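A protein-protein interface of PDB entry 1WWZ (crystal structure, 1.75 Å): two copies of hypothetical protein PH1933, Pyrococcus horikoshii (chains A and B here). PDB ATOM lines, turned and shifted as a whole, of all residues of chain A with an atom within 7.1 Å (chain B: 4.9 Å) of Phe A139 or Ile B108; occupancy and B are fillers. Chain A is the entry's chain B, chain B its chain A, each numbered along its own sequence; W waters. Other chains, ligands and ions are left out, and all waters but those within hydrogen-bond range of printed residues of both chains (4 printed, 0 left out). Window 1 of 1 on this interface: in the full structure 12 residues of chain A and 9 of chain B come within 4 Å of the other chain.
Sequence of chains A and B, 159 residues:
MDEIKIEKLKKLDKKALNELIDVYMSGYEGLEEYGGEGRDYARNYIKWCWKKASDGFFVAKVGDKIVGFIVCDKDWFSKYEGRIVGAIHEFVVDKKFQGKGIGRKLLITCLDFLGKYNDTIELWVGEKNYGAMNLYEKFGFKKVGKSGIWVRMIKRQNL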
ATOM      1  N   GLY A 103     -25.147 -27.998   4.508  1.00  0.00           N
ATOM      2  CA  GLY A 103     -24.177 -27.764   3.452  1.00  0.00           C
ATOM      3  C   GLY A 103     -22.823 -27.410   4.041  1.00  0.00           C
ATOM      4  O   GLY A 103     -21.790 -27.940   3.626  1.00  0.00           O
ATOM      5  N   ARG A 104     -22.819 -26.509   5.022  1.00  0.00           N
ATOM      6  CA  ARG A 104     -21.574 -26.112   5.667  1.00  0.00           C
ATOM      7  C   ARG A 104     -20.863 -27.327   6.255  1.00  0.00           C
ATOM      8  O   ARG A 104     -19.656 -27.480   6.094  1.00  0.00           O
ATOM      9  CB  ARG A 104     -21.853 -25.093   6.776  1.00  0.00           C
ATOM     10  CG  ARG A 104     -20.630 -24.687   7.571  1.00  0.00           C
ATOM     11  CD  ARG A 104     -21.064 -23.863   8.764  1.00  0.00           C
ATOM     12  NE  ARG A 104     -21.964 -24.639   9.610  1.00  0.00           N
ATOM     13  CZ  ARG A 104     -23.001 -24.135  10.267  1.00  0.00           C
ATOM     14  NH1 ARG A 104     -23.279 -22.841  10.182  1.00  0.00           N
ATOM     15  NH2 ARG A 104     -23.764 -24.929  11.006  1.00  0.00           N
ATOM     16  N   LYS A 105     -21.615 -28.194   6.932  1.00  0.00           N
ATOM     17  CA  LYS A 105     -21.031 -29.391   7.528  1.00  0.00           C
ATOM     18  C   LYS A 105     -20.446 -30.310   6.460  1.00  0.00           C
ATOM     19  O   LYS A 105     -19.382 -30.895   6.651  1.00  0.00           O
ATOM     20  CB  LYS A 105     -22.081 -30.152   8.349  1.00  0.00           C
ATOM     21  CG  LYS A 105     -22.497 -29.426   9.619  1.00  0.00           C
ATOM     22  CD  LYS A 105     -23.532 -30.216  10.416  1.00  0.00           C
ATOM     23  CE  LYS A 105     -23.868 -29.512  11.724  1.00  0.00           C
ATOM     24  NZ  LYS A 105     -22.671 -29.376  12.612  1.00  0.00           N
ATOM     25  N   LEU A 106     -21.138 -30.433   5.333  1.00  0.00           N
ATOM     26  CA  LEU A 106     -20.647 -31.290   4.259  1.00  0.00           C
ATOM     27  C   LEU A 106     -19.378 -30.710   3.645  1.00  0.00           C
ATOM     28  O   LEU A 106     -18.446 -31.445   3.320  1.00  0.00           O
ATOM     29  CB  LEU A 106     -21.724 -31.481   3.183  1.00  0.00           C
ATOM     30  CG  LEU A 106     -22.882 -32.412   3.579  1.00  0.00           C
ATOM     31  CD1 LEU A 106     -24.021 -32.311   2.567  1.00  0.00           C
ATOM     32  CD2 LEU A 106     -22.376 -33.846   3.672  1.00  0.00           C
ATOM     33  N   LEU A 107     -19.332 -29.389   3.494  1.00  0.00           N
ATOM     34  CA  LEU A 107     -18.158 -28.750   2.908  1.00  0.00           C
ATOM     35  C   LEU A 107     -16.963 -28.839   3.860  1.00  0.00           C
ATOM     36  O   LEU A 107     -15.831 -29.039   3.428  1.00  0.00           O
ATOM     37  CB  LEU A 107     -18.480 -27.295   2.559  1.00  0.00           C
ATOM     38  CG  LEU A 107     -17.632 -26.599   1.494  1.00  0.00           C
ATOM     39  CD1 LEU A 107     -17.532 -27.465   0.242  1.00  0.00           C
ATOM     40  CD2 LEU A 107     -18.277 -25.257   1.160  1.00  0.00           C
ATOM     41  N   ILE A 108     -17.204 -28.694   5.159  1.00  0.00           N
ATOM     42  CA  ILE A 108     -16.110 -28.817   6.121  1.00  0.00           C
ATOM     43  C   ILE A 108     -15.544 -30.230   5.996  1.00  0.00           C
ATOM     44  O   ILE A 108     -14.327 -30.431   5.989  1.00  0.00           O
ATOM     45  CB  ILE A 108     -16.594 -28.605   7.574  1.00  0.00           C
ATOM     46  CG1 ILE A 108     -16.935 -27.133   7.801  1.00  0.00           C
ATOM     47  CG2 ILE A 108     -15.521 -29.053   8.559  1.00  0.00           C
ATOM     48  CD1 ILE A 108     -17.506 -26.844   9.185  1.00  0.00           C
ATOM     49  N   THR A 109     -16.437 -31.209   5.882  1.00  0.00           N
ATOM     50  CA  THR A 109     -16.025 -32.604   5.758  1.00  0.00           C
ATOM     51  C   THR A 109     -15.209 -32.786   4.479  1.00  0.00           C
ATOM     52  O   THR A 109     -14.185 -33.470   4.468  1.00  0.00           O
ATOM     53  CB  THR A 109     -17.253 -33.539   5.721  1.00  0.00           C
ATOM     54  OG1 THR A 109     -18.006 -33.371   6.930  1.00  0.00           O
ATOM     55  CG2 THR A 109     -16.822 -35.003   5.598  1.00  0.00           C
ATOM     56  N   LEU A 111     -13.432 -30.472   2.728  1.00  0.00           N
ATOM     57  CA  LEU A 111     -12.114 -29.857   2.835  1.00  0.00           C
ATOM     58  C   LEU A 111     -11.174 -30.656   3.730  1.00  0.00           C
ATOM     59  O   LEU A 111      -9.978 -30.759   3.448  1.00  0.00           O
ATOM     60  CB  LEU A 111     -12.237 -28.421   3.343  1.00  0.00           C
ATOM     61  CG  LEU A 111     -12.304 -27.344   2.254  1.00  0.00           C
ATOM     62  CD1 LEU A 111     -13.433 -27.643   1.283  1.00  0.00           C
ATOM     63  CD2 LEU A 111     -12.487 -25.973   2.894  1.00  0.00           C
ATOM     64  N   MET A 133     -22.157 -20.116  -5.085  1.00  0.00           N
ATOM     65  CA  MET A 133     -20.935 -19.333  -5.228  1.00  0.00           C
ATOM     66  C   MET A 133     -20.619 -18.579  -3.942  1.00  0.00           C
ATOM     67  O   MET A 133     -19.463 -18.505  -3.532  1.00  0.00           O
ATOM     68  CB  MET A 133     -21.059 -18.340  -6.387  1.00  0.00           C
ATOM     69  CG  MET A 133     -21.300 -18.989  -7.736  1.00  0.00           C
ATOM     70  SD  MET A 133     -21.396 -17.768  -9.055  1.00  0.00           S
ATOM     71  CE  MET A 133     -20.096 -18.321 -10.093  1.00  0.00           C
ATOM     72  N   ASN A 134     -21.646 -18.021  -3.305  1.00  0.00           N
ATOM     73  CA  ASN A 134     -21.442 -17.287  -2.061  1.00  0.00           C
ATOM     74  C   ASN A 134     -20.856 -18.209  -0.999  1.00  0.00           C
ATOM     75  O   ASN A 134     -19.914 -17.843  -0.296  1.00  0.00           O
ATOM     76  CB  ASN A 134     -22.759 -16.704  -1.541  1.00  0.00           C
ATOM     77  CG  ASN A 134     -23.274 -15.571  -2.394  1.00  0.00           C
ATOM     78  OD1 ASN A 134     -22.498 -14.739  -2.868  1.00  0.00           O
ATOM     79  ND2 ASN A 134     -24.588 -15.513  -2.581  1.00  0.00           N
ATOM     80  N   LEU A 135     -21.421 -19.405  -0.887  1.00  0.00           N
ATOM     81  CA  LEU A 135     -20.940 -20.372   0.092  1.00  0.00           C
ATOM     82  C   LEU A 135     -19.495 -20.773  -0.203  1.00  0.00           C
ATOM     83  O   LEU A 135     -18.655 -20.806   0.697  1.00  0.00           O
ATOM     84  CB  LEU A 135     -21.839 -21.612   0.097  1.00  0.00           C
ATOM     85  CG  LEU A 135     -21.421 -22.722   1.064  1.00  0.00           C
ATOM     86  CD1 LEU A 135     -21.365 -22.168   2.476  1.00  0.00           C
ATOM     87  CD2 LEU A 135     -22.407 -23.876   0.984  1.00  0.00           C
ATOM     88  N   TYR A 136     -19.196 -21.073  -1.463  1.00  0.00           N
ATOM     89  CA  TYR A 136     -17.832 -21.459  -1.808  1.00  0.00           C
ATOM     90  C   TYR A 136     -16.849 -20.331  -1.517  1.00  0.00           C
ATOM     91  O   TYR A 136     -15.748 -20.573  -1.032  1.00  0.00           O
ATOM     92  CB  TYR A 136     -17.725 -21.846  -3.284  1.00  0.00           C
ATOM     93  CG  TYR A 136     -18.511 -23.076  -3.659  1.00  0.00           C
ATOM     94  CD1 TYR A 136     -18.487 -24.222  -2.856  1.00  0.00           C
ATOM     95  CD2 TYR A 136     -19.240 -23.118  -4.844  1.00  0.00           C
ATOM     96  CE1 TYR A 136     -19.169 -25.374  -3.235  1.00  0.00           C
ATOM     97  CE2 TYR A 136     -19.921 -24.261  -5.227  1.00  0.00           C
ATOM     98  CZ  TYR A 136     -19.882 -25.384  -4.424  1.00  0.00           C
ATOM     99  OH  TYR A 136     -20.553 -26.518  -4.821  1.00  0.00           O
ATOM    100  N   GLU A 137     -17.244 -19.099  -1.813  1.00  0.00           N
ATOM    101  CA  GLU A 137     -16.357 -17.971  -1.564  1.00  0.00           C
ATOM    102  C   GLU A 137     -16.079 -17.822  -0.068  1.00  0.00           C
ATOM    103  O   GLU A 137     -14.976 -17.451   0.329  1.00  0.00           O
ATOM    104  CB  GLU A 137     -16.951 -16.690  -2.162  1.00  0.00           C
ATOM    105  CG  GLU A 137     -17.109 -16.789  -3.681  1.00  0.00           C
ATOM    106  CD  GLU A 137     -17.496 -15.484  -4.348  1.00  0.00           C
ATOM    107  OE1 GLU A 137     -18.323 -14.745  -3.777  1.00  0.00           O
ATOM    108  OE2 GLU A 137     -16.984 -15.207  -5.455  1.00  0.00           O
ATOM    109  N   LYS A 138     -17.066 -18.133   0.764  1.00  0.00           N
ATOM    110  CA  LYS A 138     -16.860 -18.048   2.208  1.00  0.00           C
ATOM    111  C   LYS A 138     -15.835 -19.090   2.642  1.00  0.00           C
ATOM    112  O   LYS A 138     -15.108 -18.883   3.612  1.00  0.00           O
ATOM    113  CB  LYS A 138     -18.172 -18.268   2.964  1.00  0.00           C
ATOM    114  CG  LYS A 138     -19.111 -17.084   2.931  1.00  0.00           C
ATOM    115  CD  LYS A 138     -20.319 -17.336   3.818  1.00  0.00           C
ATOM    116  CE  LYS A 138     -21.264 -16.147   3.825  1.00  0.00           C
ATOM    117  NZ  LYS A 138     -22.432 -16.402   4.704  1.00  0.00           N
ATOM    118  N   PHE A 139     -15.776 -20.208   1.919  1.00  0.00           N
ATOM    119  CA  PHE A 139     -14.821 -21.262   2.237  1.00  0.00           C
ATOM    120  C   PHE A 139     -13.447 -21.059   1.592  1.00  0.00           C
ATOM    121  O   PHE A 139     -12.570 -21.914   1.713  1.00  0.00           O
ATOM    122  CB  PHE A 139     -15.379 -22.636   1.848  1.00  0.00           C
ATOM    123  CG  PHE A 139     -16.227 -23.269   2.916  1.00  0.00           C
ATOM    124  CD1 PHE A 139     -17.488 -22.763   3.218  1.00  0.00           C
ATOM    125  CD2 PHE A 139     -15.755 -24.363   3.637  1.00  0.00           C
ATOM    126  CE1 PHE A 139     -18.265 -23.339   4.227  1.00  0.00           C
ATOM    127  CE2 PHE A 139     -16.525 -24.944   4.646  1.00  0.00           C
ATOM    128  CZ  PHE A 139     -17.784 -24.428   4.940  1.00  0.00           C
ATOM    129  N   GLY A 140     -13.263 -19.938   0.900  1.00  0.00           N
ATOM    130  CA  GLY A 140     -11.969 -19.661   0.296  1.00  0.00           C
ATOM    131  C   GLY A 140     -11.819 -19.899  -1.196  1.00  0.00           C
ATOM    132  O   GLY A 140     -10.737 -19.701  -1.745  1.00  0.00           O
ATOM    133  N   PHE A 141     -12.891 -20.326  -1.853  1.00  0.00           N
ATOM    134  CA  PHE A 141     -12.841 -20.568  -3.292  1.00  0.00           C
ATOM    135  C   PHE A 141     -12.913 -19.242  -4.031  1.00  0.00           C
ATOM    136  O   PHE A 141     -13.572 -18.307  -3.573  1.00  0.00           O
ATOM    137  CB  PHE A 141     -14.009 -21.451  -3.720  1.00  0.00           C
ATOM    138  CG  PHE A 141     -13.836 -22.901  -3.358  1.00  0.00           C
ATOM    139  CD1 PHE A 141     -13.255 -23.791  -4.259  1.00  0.00           C
ATOM    140  CD2 PHE A 141     -14.246 -23.378  -2.116  1.00  0.00           C
ATOM    141  CE1 PHE A 141     -13.086 -25.136  -3.927  1.00  0.00           C
ATOM    142  CE2 PHE A 141     -14.081 -24.718  -1.774  1.00  0.00           C
ATOM    143  CZ  PHE A 141     -13.500 -25.599  -2.684  1.00  0.00           C
ATOM    144  N   LYS A 155      -9.683 -23.303  -4.914  1.00  0.00           N
ATOM    145  CA  LYS A 155      -9.232 -22.980  -3.568  1.00  0.00           C
ATOM    146  C   LYS A 155      -7.819 -23.544  -3.547  1.00  0.00           C
ATOM    147  O   LYS A 155      -7.628 -24.754  -3.681  1.00  0.00           O
ATOM    148  CB  LYS A 155     -10.064 -23.664  -2.480  1.00  0.00           C
ATOM    149  CG  LYS A 155      -9.595 -23.272  -1.072  1.00  0.00           C
ATOM    150  CD  LYS A 155     -10.327 -24.036   0.020  1.00  0.00           C
ATOM    151  CE  LYS A 155      -9.830 -23.627   1.404  1.00  0.00           C
ATOM    152  NZ  LYS A 155      -8.362 -23.845   1.548  1.00  0.00           N
ATOM    153  N   ARG B 104     -10.007 -17.896   8.381  1.00  0.00           N
ATOM    154  CA  ARG B 104     -11.275 -18.268   7.779  1.00  0.00           C
ATOM    155  C   ARG B 104     -11.700 -19.652   8.268  1.00  0.00           C
ATOM    156  O   ARG B 104     -12.859 -19.863   8.607  1.00  0.00           O
ATOM    157  CB  ARG B 104     -11.142 -18.272   6.253  1.00  0.00           C
ATOM    158  CG  ARG B 104     -12.421 -18.577   5.500  1.00  0.00           C
ATOM    159  CD  ARG B 104     -12.138 -18.704   4.006  1.00  0.00           C
ATOM    160  NE  ARG B 104     -11.678 -17.453   3.408  1.00  0.00           N
ATOM    161  CZ  ARG B 104     -12.471 -16.431   3.100  1.00  0.00           C
ATOM    162  NH1 ARG B 104     -13.775 -16.502   3.333  1.00  0.00           N
ATOM    163  NH2 ARG B 104     -11.963 -15.340   2.549  1.00  0.00           N
ATOM    164  N   LYS B 105     -10.759 -20.594   8.305  1.00  0.00           N
ATOM    165  CA  LYS B 105     -11.069 -21.952   8.754  1.00  0.00           C
ATOM    166  C   LYS B 105     -11.517 -21.969  10.208  1.00  0.00           C
ATOM    167  O   LYS B 105     -12.459 -22.677  10.578  1.00  0.00           O
ATOM    168  CB  LYS B 105      -9.858 -22.866   8.583  1.00  0.00           C
ATOM    169  CG  LYS B 105      -9.403 -23.027   7.140  1.00  0.00           C
ATOM    170  CD  LYS B 105      -8.222 -23.983   7.037  1.00  0.00           C
ATOM    171  CE  LYS B 105      -8.631 -25.413   7.352  1.00  0.00           C
ATOM    172  NZ  LYS B 105      -9.609 -25.928   6.354  1.00  0.00           N
ATOM    173  N   LEU B 106     -10.839 -21.183  11.033  1.00  0.00           N
ATOM    174  CA  LEU B 106     -11.188 -21.112  12.441  1.00  0.00           C
ATOM    175  C   LEU B 106     -12.565 -20.484  12.625  1.00  0.00           C
ATOM    176  O   LEU B 106     -13.345 -20.942  13.454  1.00  0.00           O
ATOM    177  CB  LEU B 106     -10.129 -20.312  13.209  1.00  0.00           C
ATOM    178  CG  LEU B 106      -8.813 -21.048  13.501  1.00  0.00           C
ATOM    179  CD1 LEU B 106      -7.776 -20.062  14.005  1.00  0.00           C
ATOM    180  CD2 LEU B 106      -9.050 -22.155  14.532  1.00  0.00           C
ATOM    181  N   LEU B 107     -12.870 -19.445  11.845  1.00  0.00           N
ATOM    182  CA  LEU B 107     -14.164 -18.778  11.967  1.00  0.00           C
ATOM    183  C   LEU B 107     -15.307 -19.691  11.536  1.00  0.00           C
ATOM    184  O   LEU B 107     -16.351 -19.742  12.189  1.00  0.00           O
ATOM    185  CB  LEU B 107     -14.175 -17.475  11.158  1.00  0.00           C
ATOM    186  CG  LEU B 107     -15.402 -16.563  11.308  1.00  0.00           C
ATOM    187  CD1 LEU B 107     -15.670 -16.273  12.785  1.00  0.00           C
ATOM    188  CD2 LEU B 107     -15.160 -15.265  10.547  1.00  0.00           C
ATOM    189  N   ILE B 108     -15.111 -20.416  10.439  1.00  0.00           N
ATOM    190  CA  ILE B 108     -16.127 -21.345   9.959  1.00  0.00           C
ATOM    191  C   ILE B 108     -16.367 -22.418  11.026  1.00  0.00           C
ATOM    192  O   ILE B 108     -17.506 -22.792  11.300  1.00  0.00           O
ATOM    193  CB  ILE B 108     -15.683 -22.004   8.632  1.00  0.00           C
ATOM    194  CG1 ILE B 108     -15.726 -20.955   7.513  1.00  0.00           C
ATOM    195  CG2 ILE B 108     -16.578 -23.198   8.302  1.00  0.00           C
ATOM    196  CD1 ILE B 108     -15.165 -21.436   6.175  1.00  0.00           C
ATOM    197  N   THR B 109     -15.285 -22.898  11.632  1.00  0.00           N
ATOM    198  CA  THR B 109     -15.379 -23.904  12.682  1.00  0.00           C
ATOM    199  C   THR B 109     -16.190 -23.332  13.840  1.00  0.00           C
ATOM    200  O   THR B 109     -17.045 -24.010  14.413  1.00  0.00           O
ATOM    201  CB  THR B 109     -13.982 -24.299  13.192  1.00  0.00           C
ATOM    202  OG1 THR B 109     -13.243 -24.903  12.125  1.00  0.00           O
ATOM    203  CG2 THR B 109     -14.085 -25.288  14.349  1.00  0.00           C
ATOM    204  N   CYS B 110     -15.909 -22.079  14.177  1.00  0.00           N
ATOM    205  CA  CYS B 110     -16.613 -21.396  15.256  1.00  0.00           C
ATOM    206  C   CYS B 110     -18.107 -21.263  14.966  1.00  0.00           C
ATOM    207  O   CYS B 110     -18.945 -21.527  15.830  1.00  0.00           O
ATOM    208  CB  CYS B 110     -16.016 -20.003  15.471  1.00  0.00           C
ATOM    209  SG  CYS B 110     -16.997 -18.940  16.561  1.00  0.00           S
ATOM    210  N   LEU B 111     -18.442 -20.851  13.746  1.00  0.00           N
ATOM    211  CA  LEU B 111     -19.841 -20.683  13.374  1.00  0.00           C
ATOM    212  C   LEU B 111     -20.596 -22.005  13.420  1.00  0.00           C
ATOM    213  O   LEU B 111     -21.748 -22.050  13.857  1.00  0.00           O
ATOM    214  CB  LEU B 111     -19.954 -20.054  11.980  1.00  0.00           C
ATOM    215  CG  LEU B 111     -19.430 -18.618  11.867  1.00  0.00           C
ATOM    216  CD1 LEU B 111     -19.802 -18.036  10.513  1.00  0.00           C
ATOM    217  CD2 LEU B 111     -20.024 -17.764  12.969  1.00  0.00           C
ATOM    218  N   ASP B 112     -19.941 -23.076  12.981  1.00  0.00           N
ATOM    219  CA  ASP B 112     -20.548 -24.402  12.984  1.00  0.00           C
ATOM    220  C   ASP B 112     -20.747 -24.888  14.419  1.00  0.00           C
ATOM    221  O   ASP B 112     -21.786 -25.447  14.757  1.00  0.00           O
ATOM    222  CB  ASP B 112     -19.658 -25.390  12.225  1.00  0.00           C
ATOM    223  CG  ASP B 112     -20.215 -26.797  12.233  1.00  0.00           C
ATOM    224  OD1 ASP B 112     -21.237 -27.041  11.562  1.00  0.00           O
ATOM    225  OD2 ASP B 112     -19.633 -27.660  12.922  1.00  0.00           O
ATOM    226  N   PHE B 139     -18.932 -12.709   6.717  1.00  0.00           N
ATOM    227  CA  PHE B 139     -19.607 -13.873   7.258  1.00  0.00           C
ATOM    228  C   PHE B 139     -20.959 -13.550   7.873  1.00  0.00           C
ATOM    229  O   PHE B 139     -21.532 -14.363   8.594  1.00  0.00           O
ATOM    230  CB  PHE B 139     -18.701 -14.573   8.269  1.00  0.00           C
ATOM    231  CG  PHE B 139     -17.701 -15.484   7.628  1.00  0.00           C
ATOM    232  CD1 PHE B 139     -18.004 -16.826   7.416  1.00  0.00           C
ATOM    233  CD2 PHE B 139     -16.485 -14.990   7.167  1.00  0.00           C
ATOM    234  CE1 PHE B 139     -17.113 -17.665   6.750  1.00  0.00           C
ATOM    235  CE2 PHE B 139     -15.586 -15.820   6.498  1.00  0.00           C
ATOM    236  CZ  PHE B 139     -15.901 -17.161   6.290  1.00  0.00           C
HETATM  237  O   HOH W   1      -9.923 -28.629   6.115  1.00  0.00           O
HETATM  238  O   HOH W   2     -23.930 -26.000  13.499  1.00  0.00           O
HETATM  239  O   HOH W   3      -8.629 -25.823   3.784  1.00  0.00           O
HETATM  240  O   HOH W   4     -21.073 -29.179  15.168  1.00  0.00           O
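O of Glu A137 is in hydrogen-bond range of NH1 of Arg B104, 3.4 Å away. The guanidinium group (NH1) of Arg B104 sits at hydrogen-bond distance from the backbone carbonyl oxygen (O) of Lys A138 (2.7 Å). The side-chain carboxylate (OD1) of Asp B112 is in salt-bridge range of the guanidinium group (NE) of Arg A104, 3.2 Å away. NZ of Lys A105 is in salt-bridge range of OD1 of Asp B112, at 2.9 Å.
O of Lys A105 sits at hydrogen-bond distance from OG1 of Thr A109, 2.8 Å away.
Among the printed residues, merely in contact across the chains: Lys A138 with Phe B139 (3.3 Å), Gly A140 with Arg B104 (3.5 Å), Phe A139 with Arg B104 (3.6 Å), Lys A138 with Ile B108 (3.6 Å), Phe A139 with Ile B108 (3.8 Å), Ile A108 with Ile B108 (3.9 Å) and Ile A108 with Asp B112 (3.998 Å).
Phe A139 touches just these residues of chain B: Arg B104 and Ile B108. Ile B108 touches just these residues of chain A: Ile A108, Lys A138 and Phe A139. Printed residues of chain B within 4 Å of Glu A137: Arg B104. Of the printed residues of chain A, Arg B104 touches Glu A137, Lys A138, Phe A139 and Gly A140. Leu A107 touches none of the printed residues of chain B. The nearest printed residue of chain B that does not touch Phe A139 is Phe B139 (5.3 Å). The nearest residue of chain A that does not touch Ile B108 is Arg A104 (4.4 Å).
Of the 10 printed residues of chain B, 4 touch a printed residue of chain A. Of the 18 printed residues of chain A, 7 touch a printed residue of chain B. Printed residues of chain A that touch a printed residue of chain B: Arg A104, Lys A105, Ile A108, Glu A137, Lys A138, Phe A139 and Gly A140. Hydrophobic or aromatic side chains of chain A within 4 Å of the printed part of chain B: Ile A108 and Phe A139. Along chain A the printed residues that touch a printed residue of chain B span positions 104 to 140. Among the printed residues, Asp or Glu carboxylates within 4 Å of a Lys or Arg side-chain nitrogen of the other chain: Arg A104 with Asp B112 (3.2 Å) and Lys A105 with Asp B112 (2.9 Å).
Ile B108 touches its own counterpart, Ile A108. Phe A139 touches Arg B104, but with the chains exchanged Arg A104 does not touch Phe B139 (7.6 Å). Phe A139 touches Ile B108, but with the chains exchanged Ile A108 does not touch Phe B139 (9.5 Å). 8 positions are printed for both chains.
Water W2 lies within hydrogen-bond range of O of Asp B112 (2.5 Å) and NH2 of Arg A104 (2.7 Å). Water W1 lies within hydrogen-bond range of NZ of Lys B105 and O of Leu A111. Water W3 lies within hydrogen-bond range of NZ of Lys B105 (2.8 Å) and NZ of Lys A155 (3.0 Å). Water W4 bridges the side-chain amino group of Lys A105 (3.0 Å) and the side-chain carboxylate of Asp B112 (3.1 Å).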
